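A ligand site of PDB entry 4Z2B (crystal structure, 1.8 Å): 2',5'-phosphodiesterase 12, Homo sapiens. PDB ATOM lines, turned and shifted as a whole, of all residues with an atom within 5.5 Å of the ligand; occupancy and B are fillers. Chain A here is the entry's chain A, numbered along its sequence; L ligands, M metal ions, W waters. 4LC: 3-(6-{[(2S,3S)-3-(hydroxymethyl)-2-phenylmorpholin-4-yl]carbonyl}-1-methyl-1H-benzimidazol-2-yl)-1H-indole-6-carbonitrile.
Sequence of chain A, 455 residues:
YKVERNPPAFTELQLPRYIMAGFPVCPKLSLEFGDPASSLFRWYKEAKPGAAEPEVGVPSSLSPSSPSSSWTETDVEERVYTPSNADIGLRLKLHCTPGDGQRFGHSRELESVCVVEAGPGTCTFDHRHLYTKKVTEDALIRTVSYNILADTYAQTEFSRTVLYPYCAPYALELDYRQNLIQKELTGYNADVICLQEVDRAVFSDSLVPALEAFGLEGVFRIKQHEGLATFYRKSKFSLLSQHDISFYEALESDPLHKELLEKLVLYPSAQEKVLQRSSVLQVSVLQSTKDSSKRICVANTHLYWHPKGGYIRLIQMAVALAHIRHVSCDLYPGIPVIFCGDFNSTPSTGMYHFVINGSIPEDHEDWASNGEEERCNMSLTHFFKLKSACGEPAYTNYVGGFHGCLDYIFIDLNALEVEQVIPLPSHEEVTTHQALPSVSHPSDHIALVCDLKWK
A nitrogen (N62) of the ligand is in hydrogen-bond range of the backbone NH (N) of Thr 346.
An oxygen (O34) of the ligand is in hydrogen-bond range of the side-chain carboxylate (OE2) of Glu 197 (2.6 Å).
The guanidinium group (NH1) of Arg 313 sits at hydrogen-bond distance from the backbone carbonyl oxygen (O) of Pro 307 (3.4 Å).
The backbone NH of Leu 163 is in hydrogen-bond range of the backbone carbonyl oxygen of Phe 158.
N of Ser 159 lies within hydrogen-bond range of OG1 of Thr 156 (3.1 Å).
OE2 of Glu 197 lies within hydrogen-bond range of ND2 of Asn 147 (3.0 Å).
The backbone carbonyl oxygen (O) of Thr 346 sits at hydrogen-bond distance from the side-chain hydroxyl (OG1) of Thr 349 (2.8 Å).
The side-chain hydroxyl of Ser 159 sits at hydrogen-bond distance from the backbone carbonyl oxygen of Tyr 153, 2.7 Å away.
The backbone carbonyl oxygen (O) of Ser 159 is in hydrogen-bond range of the backbone NH (N) of Tyr 164 (2.8 Å).
NE of Arg 313 is in hydrogen-bond range of O of Asn 344 (2.9 Å).
Residues that only touch the ligand: Trp 305 (3.2 Å), Asn 344 (3.2 Å), Phe 402 (3.2 Å), Ser 159 (3.3 Å), Tyr 153 (3.4 Å), Thr 156 (3.5 Å), Thr 349 (3.5 Å), Ser 345 (3.6 Å), Pro 307 (3.7 Å), Phe 158 (3.7 Å), Leu 163 (3.9 Å) and Arg 313 (3.9 Å).
Within 4 Å of the ligand: Tyr 153, Thr 156, Phe 158, Ser 159, Leu 163, Glu 197, Trp 305, Pro 307, Arg 313, Asn 344, Ser 345, Thr 346, Thr 349 and Phe 402.
The nearest printed residue that does not touch the ligand is Leu 406 (4.001 Å).
Water W7 lies within hydrogen-bond range of O34 of the ligand (2.7 Å), NE2 of His 302 (2.9 Å) and ND2 of Asn 344 (3.1 Å).
Water W5 lies within hydrogen-bond range of OD2 of Asp 444 (2.7 Å), O18 of the ligand (2.9 Å) and OH of Tyr 164 (3.0 Å).
Water W1 lies within hydrogen-bond range of NH1 of Arg 313 (3.0 Å) and N62 of the ligand (3.0 Å).
Water W2 bridges the side-chain carboxylate of Glu 197 (2.7 Å) and an oxygen (O34) of the ligand (3.1 Å).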
ATOM      1  N   ASN A 147       4.349  -7.754   6.474  1.00  0.00           N
ATOM      2  CA  ASN A 147       3.024  -7.726   7.065  1.00  0.00           C
ATOM      3  C   ASN A 147       2.100  -7.912   5.879  1.00  0.00           C
ATOM      4  O   ASN A 147       2.026  -7.024   5.025  1.00  0.00           O
ATOM      5  CB  ASN A 147       2.769  -6.411   7.817  1.00  0.00           C
ATOM      6  CG  ASN A 147       1.384  -6.401   8.433  1.00  0.00           C
ATOM      7  OD1 ASN A 147       0.409  -6.941   7.868  1.00  0.00           O
ATOM      8  ND2 ASN A 147       1.255  -5.757   9.583  1.00  0.00           N
ATOM      9  N   TYR A 153      -8.961  -8.577   9.289  1.00  0.00           N
ATOM     10  CA  TYR A 153      -9.059  -7.126   9.310  1.00  0.00           C
ATOM     11  C   TYR A 153      -9.533  -6.560   7.975  1.00  0.00           C
ATOM     12  O   TYR A 153     -10.364  -5.654   7.960  1.00  0.00           O
ATOM     13  CB  TYR A 153      -7.717  -6.465   9.706  1.00  0.00           C
ATOM     14  CG  TYR A 153      -7.124  -7.036  10.967  1.00  0.00           C
ATOM     15  CD1 TYR A 153      -7.928  -7.304  12.080  1.00  0.00           C
ATOM     16  CD2 TYR A 153      -5.788  -7.415  11.030  1.00  0.00           C
ATOM     17  CE1 TYR A 153      -7.388  -7.811  13.253  1.00  0.00           C
ATOM     18  CE2 TYR A 153      -5.239  -7.969  12.186  1.00  0.00           C
ATOM     19  CZ  TYR A 153      -6.051  -8.178  13.287  1.00  0.00           C
ATOM     20  OH  TYR A 153      -5.566  -8.682  14.457  1.00  0.00           O
ATOM     21  N   THR A 156     -13.419  -6.144   7.263  1.00  0.00           N
ATOM     22  CA  THR A 156     -14.258  -5.252   8.079  1.00  0.00           C
ATOM     23  C   THR A 156     -14.717  -4.049   7.268  1.00  0.00           C
ATOM     24  O   THR A 156     -14.014  -3.649   6.336  1.00  0.00           O
ATOM     25  CB  THR A 156     -13.514  -4.768   9.323  1.00  0.00           C
ATOM     26  OG1 THR A 156     -12.408  -3.942   8.936  1.00  0.00           O
ATOM     27  CG2 THR A 156     -13.047  -5.915  10.231  1.00  0.00           C
ATOM     28  N   PHE A 158     -14.708  -0.965   8.375  1.00  0.00           N
ATOM     29  CA  PHE A 158     -13.691   0.027   8.667  1.00  0.00           C
ATOM     30  C   PHE A 158     -12.529  -0.105   7.646  1.00  0.00           C
ATOM     31  O   PHE A 158     -12.113   0.903   7.086  1.00  0.00           O
ATOM     32  CB  PHE A 158     -13.198  -0.138  10.112  1.00  0.00           C
ATOM     33  CG  PHE A 158     -12.120   0.837  10.547  1.00  0.00           C
ATOM     34  CD1 PHE A 158     -12.439   2.173  10.802  1.00  0.00           C
ATOM     35  CD2 PHE A 158     -10.809   0.428  10.732  1.00  0.00           C
ATOM     36  CE1 PHE A 158     -11.453   3.071  11.218  1.00  0.00           C
ATOM     37  CE2 PHE A 158      -9.833   1.317  11.178  1.00  0.00           C
ATOM     38  CZ  PHE A 158     -10.152   2.632  11.420  1.00  0.00           C
ATOM     39  N   SER A 159     -12.030  -1.344   7.352  1.00  0.00           N
ATOM     40  CA  SER A 159     -10.937  -1.448   6.373  1.00  0.00           C
ATOM     41  C   SER A 159     -11.426  -1.132   4.947  1.00  0.00           C
ATOM     42  O   SER A 159     -10.777  -0.382   4.216  1.00  0.00           O
ATOM     43  CB  SER A 159     -10.298  -2.838   6.379  1.00  0.00           C
ATOM     44  OG  SER A 159      -9.632  -3.076   7.602  1.00  0.00           O
ATOM     45  N   LEU A 163     -10.245   2.734   5.845  1.00  0.00           N
ATOM     46  CA  LEU A 163      -8.801   2.594   5.592  1.00  0.00           C
ATOM     47  C   LEU A 163      -8.441   2.529   4.102  1.00  0.00           C
ATOM     48  O   LEU A 163      -7.552   3.238   3.654  1.00  0.00           O
ATOM     49  CB  LEU A 163      -8.251   1.335   6.304  1.00  0.00           C
ATOM     50  CG  LEU A 163      -8.234   1.334   7.844  1.00  0.00           C
ATOM     51  CD1 LEU A 163      -7.631   0.043   8.363  1.00  0.00           C
ATOM     52  CD2 LEU A 163      -7.448   2.541   8.433  1.00  0.00           C
ATOM     53  N   TYR A 164      -9.111   1.658   3.329  1.00  0.00           N
ATOM     54  CA  TYR A 164      -8.756   1.447   1.923  1.00  0.00           C
ATOM     55  C   TYR A 164      -9.946   1.684   0.942  1.00  0.00           C
ATOM     56  O   TYR A 164     -10.162   0.823   0.078  1.00  0.00           O
ATOM     57  CB  TYR A 164      -8.193   0.018   1.720  1.00  0.00           C
ATOM     58  CG  TYR A 164      -7.411  -0.544   2.899  1.00  0.00           C
ATOM     59  CD1 TYR A 164      -6.242   0.082   3.341  1.00  0.00           C
ATOM     60  CD2 TYR A 164      -7.820  -1.715   3.529  1.00  0.00           C
ATOM     61  CE1 TYR A 164      -5.527  -0.422   4.434  1.00  0.00           C
ATOM     62  CE2 TYR A 164      -7.084  -2.259   4.594  1.00  0.00           C
ATOM     63  CZ  TYR A 164      -5.951  -1.595   5.045  1.00  0.00           C
ATOM     64  OH  TYR A 164      -5.251  -2.103   6.129  1.00  0.00           O
ATOM     65  N   GLU A 197       0.487 -10.799  10.458  1.00  0.00           N
ATOM     66  CA  GLU A 197      -0.949 -10.747  10.070  1.00  0.00           C
ATOM     67  C   GLU A 197      -1.307 -11.916   9.173  1.00  0.00           C
ATOM     68  O   GLU A 197      -1.971 -11.769   8.131  1.00  0.00           O
ATOM     69  CB  GLU A 197      -1.317  -9.399   9.419  1.00  0.00           C
ATOM     70  CG  GLU A 197      -1.304  -8.246  10.415  1.00  0.00           C
ATOM     71  CD  GLU A 197      -2.021  -6.985   9.955  1.00  0.00           C
ATOM     72  OE1 GLU A 197      -2.936  -7.079   9.104  1.00  0.00           O
ATOM     73  OE2 GLU A 197      -1.646  -5.892  10.435  1.00  0.00           O
ATOM     74  N   HIS A 302       5.187  -8.347  15.767  1.00  0.00           N
ATOM     75  CA  HIS A 302       4.217  -7.369  15.331  1.00  0.00           C
ATOM     76  C   HIS A 302       3.820  -6.588  16.570  1.00  0.00           C
ATOM     77  O   HIS A 302       3.095  -7.103  17.420  1.00  0.00           O
ATOM     78  CB  HIS A 302       3.018  -8.040  14.633  1.00  0.00           C
ATOM     79  CG  HIS A 302       2.022  -7.082  14.036  1.00  0.00           C
ATOM     80  ND1 HIS A 302       0.785  -7.513  13.595  1.00  0.00           N
ATOM     81  CD2 HIS A 302       2.113  -5.744  13.828  1.00  0.00           C
ATOM     82  CE1 HIS A 302       0.171  -6.440  13.120  1.00  0.00           C
ATOM     83  NE2 HIS A 302       0.905  -5.344  13.296  1.00  0.00           N
ATOM     84  N   TRP A 305      -0.226  -1.467  17.492  1.00  0.00           N
ATOM     85  CA  TRP A 305      -0.501  -0.597  16.345  1.00  0.00           C
ATOM     86  C   TRP A 305      -0.700   0.903  16.627  1.00  0.00           C
ATOM     87  O   TRP A 305      -0.565   1.692  15.696  1.00  0.00           O
ATOM     88  CB  TRP A 305      -1.806  -1.075  15.632  1.00  0.00           C
ATOM     89  CG  TRP A 305      -3.047  -0.793  16.448  1.00  0.00           C
ATOM     90  CD1 TRP A 305      -3.542  -1.537  17.486  1.00  0.00           C
ATOM     91  CD2 TRP A 305      -3.905   0.362  16.346  1.00  0.00           C
ATOM     92  NE1 TRP A 305      -4.650  -0.921  18.025  1.00  0.00           N
ATOM     93  CE2 TRP A 305      -4.889   0.249  17.357  1.00  0.00           C
ATOM     94  CE3 TRP A 305      -3.936   1.495  15.498  1.00  0.00           C
ATOM     95  CZ2 TRP A 305      -5.891   1.218  17.542  1.00  0.00           C
ATOM     96  CZ3 TRP A 305      -4.952   2.439  15.661  1.00  0.00           C
ATOM     97  CH2 TRP A 305      -5.917   2.295  16.676  1.00  0.00           C
ATOM     98  N   HIS A 306      -1.208   1.298  17.819  1.00  0.00           N
ATOM     99  CA  HIS A 306      -1.720   2.658  18.049  1.00  0.00           C
ATOM    100  C   HIS A 306      -0.688   3.751  17.774  1.00  0.00           C
ATOM    101  O   HIS A 306       0.457   3.660  18.240  1.00  0.00           O
ATOM    102  CB  HIS A 306      -2.325   2.806  19.445  1.00  0.00           C
ATOM    103  CG  HIS A 306      -3.242   3.968  19.624  1.00  0.00           C
ATOM    104  ND1 HIS A 306      -2.764   5.255  19.822  1.00  0.00           N
ATOM    105  CD2 HIS A 306      -4.602   4.010  19.653  1.00  0.00           C
ATOM    106  CE1 HIS A 306      -3.831   6.028  19.930  1.00  0.00           C
ATOM    107  NE2 HIS A 306      -4.964   5.313  19.868  1.00  0.00           N
ATOM    108  N   PRO A 307      -1.078   4.821  16.999  1.00  0.00           N
ATOM    109  CA  PRO A 307      -0.106   5.888  16.698  1.00  0.00           C
ATOM    110  C   PRO A 307       0.534   6.507  17.950  1.00  0.00           C
ATOM    111  O   PRO A 307       1.668   6.943  17.896  1.00  0.00           O
ATOM    112  CB  PRO A 307      -0.948   6.931  15.931  1.00  0.00           C
ATOM    113  CG  PRO A 307      -2.382   6.589  16.254  1.00  0.00           C
ATOM    114  CD  PRO A 307      -2.377   5.083  16.349  1.00  0.00           C
ATOM    115  N   ARG A 313       5.322   0.137  22.832  1.00  0.00           N
ATOM    116  CA  ARG A 313       6.297  -0.457  21.906  1.00  0.00           C
ATOM    117  C   ARG A 313       7.663  -0.505  22.525  1.00  0.00           C
ATOM    118  O   ARG A 313       8.395  -1.469  22.300  1.00  0.00           O
ATOM    119  CB  ARG A 313       6.334   0.306  20.597  1.00  0.00           C
ATOM    120  CG  ARG A 313       5.052   0.087  19.803  1.00  0.00           C
ATOM    121  CD  ARG A 313       5.106   0.799  18.467  1.00  0.00           C
ATOM    122  NE  ARG A 313       4.823   2.244  18.518  1.00  0.00           N
ATOM    123  CZ  ARG A 313       3.595   2.757  18.357  1.00  0.00           C
ATOM    124  NH1 ARG A 313       3.426   4.069  18.318  1.00  0.00           N
ATOM    125  NH2 ARG A 313       2.550   1.942  18.222  1.00  0.00           N
ATOM    126  N   ASN A 344       5.736  -0.992  13.981  1.00  0.00           N
ATOM    127  CA  ASN A 344       4.814   0.139  14.147  1.00  0.00           C
ATOM    128  C   ASN A 344       5.572   1.345  14.770  1.00  0.00           C
ATOM    129  O   ASN A 344       5.023   2.060  15.612  1.00  0.00           O
ATOM    130  CB  ASN A 344       3.598  -0.286  14.993  1.00  0.00           C
ATOM    131  CG  ASN A 344       2.522  -0.868  14.140  1.00  0.00           C
ATOM    132  OD1 ASN A 344       2.217  -0.300  13.080  1.00  0.00           O
ATOM    133  ND2 ASN A 344       1.934  -2.007  14.541  1.00  0.00           N
ATOM    134  N   SER A 345       6.857   1.530  14.362  1.00  0.00           N
ATOM    135  CA  SER A 345       7.725   2.573  14.881  1.00  0.00           C
ATOM    136  C   SER A 345       8.557   3.180  13.777  1.00  0.00           C
ATOM    137  O   SER A 345       9.291   2.468  13.107  1.00  0.00           O
ATOM    138  CB  SER A 345       8.656   2.017  15.953  1.00  0.00           C
ATOM    139  OG  SER A 345       7.982   1.302  16.964  1.00  0.00           O
ATOM    140  N   THR A 346       8.468   4.498  13.608  1.00  0.00           N
ATOM    141  CA  THR A 346       9.268   5.201  12.591  1.00  0.00           C
ATOM    142  C   THR A 346      10.686   5.455  13.120  1.00  0.00           C
ATOM    143  O   THR A 346      10.895   5.457  14.344  1.00  0.00           O
ATOM    144  CB  THR A 346       8.579   6.506  12.113  1.00  0.00           C
ATOM    145  OG1 THR A 346       8.580   7.428  13.182  1.00  0.00           O
ATOM    146  CG2 THR A 346       7.165   6.283  11.587  1.00  0.00           C
ATOM    147  N   THR A 349      11.428   7.696  16.370  1.00  0.00           N
ATOM    148  CA  THR A 349      10.795   7.370  17.659  1.00  0.00           C
ATOM    149  C   THR A 349      11.766   6.864  18.702  1.00  0.00           C
ATOM    150  O   THR A 349      12.910   6.489  18.402  1.00  0.00           O
ATOM    151  CB  THR A 349       9.696   6.309  17.458  1.00  0.00           C
ATOM    152  OG1 THR A 349      10.333   5.078  17.109  1.00  0.00           O
ATOM    153  CG2 THR A 349       8.652   6.714  16.441  1.00  0.00           C
ATOM    154  N   ASN A 397       4.813   1.319   4.741  1.00  0.00           N
ATOM    155  CA  ASN A 397       3.370   1.232   4.935  1.00  0.00           C
ATOM    156  C   ASN A 397       2.826   2.471   4.311  1.00  0.00           C
ATOM    157  O   ASN A 397       3.295   3.567   4.618  1.00  0.00           O
ATOM    158  CB  ASN A 397       3.043   1.114   6.448  1.00  0.00           C
ATOM    159  CG  ASN A 397       1.567   1.218   6.792  1.00  0.00           C
ATOM    160  OD1 ASN A 397       1.186   2.010   7.645  1.00  0.00           O
ATOM    161  ND2 ASN A 397       0.715   0.464   6.145  1.00  0.00           N
ATOM    162  N   PHE A 402      -2.293   7.503   6.307  1.00  0.00           N
ATOM    163  CA  PHE A 402      -0.959   7.558   6.923  1.00  0.00           C
ATOM    164  C   PHE A 402       0.061   6.819   6.054  1.00  0.00           C
ATOM    165  O   PHE A 402      -0.295   5.924   5.303  1.00  0.00           O
ATOM    166  CB  PHE A 402      -0.968   6.940   8.347  1.00  0.00           C
ATOM    167  CG  PHE A 402       0.387   6.537   8.913  1.00  0.00           C
ATOM    168  CD1 PHE A 402       1.238   7.495   9.484  1.00  0.00           C
ATOM    169  CD2 PHE A 402       0.825   5.221   8.850  1.00  0.00           C
ATOM    170  CE1 PHE A 402       2.500   7.129   9.984  1.00  0.00           C
ATOM    171  CE2 PHE A 402       2.098   4.862   9.329  1.00  0.00           C
ATOM    172  CZ  PHE A 402       2.914   5.813   9.913  1.00  0.00           C
ATOM    173  N   LEU A 406       7.757   1.533   9.097  1.00  0.00           N
ATOM    174  CA  LEU A 406       7.349   0.814  10.321  1.00  0.00           C
ATOM    175  C   LEU A 406       7.977  -0.540  10.496  1.00  0.00           C
ATOM    176  O   LEU A 406       7.916  -1.100  11.599  1.00  0.00           O
ATOM    177  CB  LEU A 406       5.826   0.603  10.296  1.00  0.00           C
ATOM    178  CG  LEU A 406       4.953   1.855  10.178  1.00  0.00           C
ATOM    179  CD1 LEU A 406       3.507   1.466  10.162  1.00  0.00           C
ATOM    180  CD2 LEU A 406       5.260   2.855  11.283  1.00  0.00           C
ATOM    181  N   ASP A 444      -1.099  -3.439   2.779  1.00  0.00           N
ATOM    182  CA  ASP A 444      -0.900  -2.008   3.037  1.00  0.00           C
ATOM    183  C   ASP A 444       0.575  -1.764   3.346  1.00  0.00           C
ATOM    184  O   ASP A 444       1.022  -0.616   3.388  1.00  0.00           O
ATOM    185  CB  ASP A 444      -1.824  -1.496   4.150  1.00  0.00           C
ATOM    186  CG  ASP A 444      -1.734  -2.250   5.466  1.00  0.00           C
ATOM    187  OD1 ASP A 444      -1.384  -3.431   5.450  1.00  0.00           O
ATOM    188  OD2 ASP A 444      -2.086  -1.660   6.492  1.00  0.00           O
HETATM  189  C13 4LC L   1      -4.273   0.029  11.640  1.00  0.00           C
HETATM  190  C17 4LC L   1      -4.625  -1.393  11.309  1.00  0.00           C
HETATM  191  C20 4LC L   1      -4.728  -1.834  13.740  1.00  0.00           C
HETATM  192  C01 4LC L   1      -0.060   1.662  11.963  1.00  0.00           C
HETATM  193  N05 4LC L   1      -1.362   2.326  12.144  1.00  0.00           N
HETATM  194  C06 4LC L   1      -1.642   3.602  12.529  1.00  0.00           C
HETATM  195  N07 4LC L   1      -2.939   3.884  12.499  1.00  0.00           N
HETATM  196  C08 4LC L   1      -3.550   2.665  12.193  1.00  0.00           C
HETATM  197  C09 4LC L   1      -4.897   2.324  12.111  1.00  0.00           C
HETATM  198  C11 4LC L   1      -5.248   1.021  11.795  1.00  0.00           C
HETATM  199  C14 4LC L   1      -2.920   0.356  11.730  1.00  0.00           C
HETATM  200  C16 4LC L   1      -2.579   1.678  11.999  1.00  0.00           C
HETATM  201  O18 4LC L   1      -4.691  -1.750  10.146  1.00  0.00           O
HETATM  202  N19 4LC L   1      -4.854  -2.257  12.332  1.00  0.00           N
HETATM  203  C23 4LC L   1      -5.941  -2.278  14.523  1.00  0.00           C
HETATM  204  O26 4LC L   1      -6.109  -3.702  14.424  1.00  0.00           O
HETATM  205  C27 4LC L   1      -6.263  -4.160  13.076  1.00  0.00           C
HETATM  206  C29 4LC L   1      -5.099  -3.708  12.178  1.00  0.00           C
HETATM  207  C31 4LC L   1      -3.828  -4.533  12.426  1.00  0.00           C
HETATM  208  O34 4LC L   1      -2.709  -3.967  11.751  1.00  0.00           O
HETATM  209  C36 4LC L   1      -7.666  -3.839  12.576  1.00  0.00           C
HETATM  210  C37 4LC L   1      -8.778  -4.258  13.300  1.00  0.00           C
HETATM  211  C39 4LC L   1     -10.065  -4.015  12.838  1.00  0.00           C
HETATM  212  C41 4LC L   1     -10.267  -3.341  11.657  1.00  0.00           C
HETATM  213  C43 4LC L   1      -9.175  -2.933  10.904  1.00  0.00           C
HETATM  214  C45 4LC L   1      -7.884  -3.167  11.367  1.00  0.00           C
HETATM  215  C47 4LC L   1      -0.650   4.672  12.662  1.00  0.00           C
HETATM  216  C48 4LC L   1      -0.735   5.938  12.131  1.00  0.00           C
HETATM  217  N50 4LC L   1       0.371   6.667  12.461  1.00  0.00           N
HETATM  218  C52 4LC L   1       1.267   5.861  13.120  1.00  0.00           C
HETATM  219  C53 4LC L   1       2.548   6.125  13.595  1.00  0.00           C
HETATM  220  C55 4LC L   1       3.219   5.120  14.295  1.00  0.00           C
HETATM  221  C56 4LC L   1       2.620   3.879  14.512  1.00  0.00           C
HETATM  222  C58 4LC L   1       1.325   3.631  14.040  1.00  0.00           C
HETATM  223  C60 4LC L   1       0.632   4.614  13.330  1.00  0.00           C
HETATM  224  C61 4LC L   1       4.577   5.353  14.727  1.00  0.00           C
HETATM  225  N62 4LC L   1       5.649   5.504  15.050  1.00  0.00           N
HETATM  226 MG    MG M   1      -2.693  -3.002   8.878  1.00  0.00          MG
HETATM  227  O   HOH W   1       5.559   6.140  18.020  1.00  0.00           O
HETATM  228  O   HOH W   2      -4.120  -4.659   9.076  1.00  0.00           O
HETATM  229  O   HOH W   3       5.317   8.455  16.310  1.00  0.00           O
HETATM  230  O   HOH W   4      -0.199   9.333  11.887  1.00  0.00           O
HETATM  231  O   HOH W   5      -3.799  -0.154   7.932  1.00  0.00           O
HETATM  232  O   HOH W   6      -3.816   6.335  13.150  1.00  0.00           O
HETATM  233  O   HOH W   7      -0.489  -2.821  12.869  1.00  0.00           O
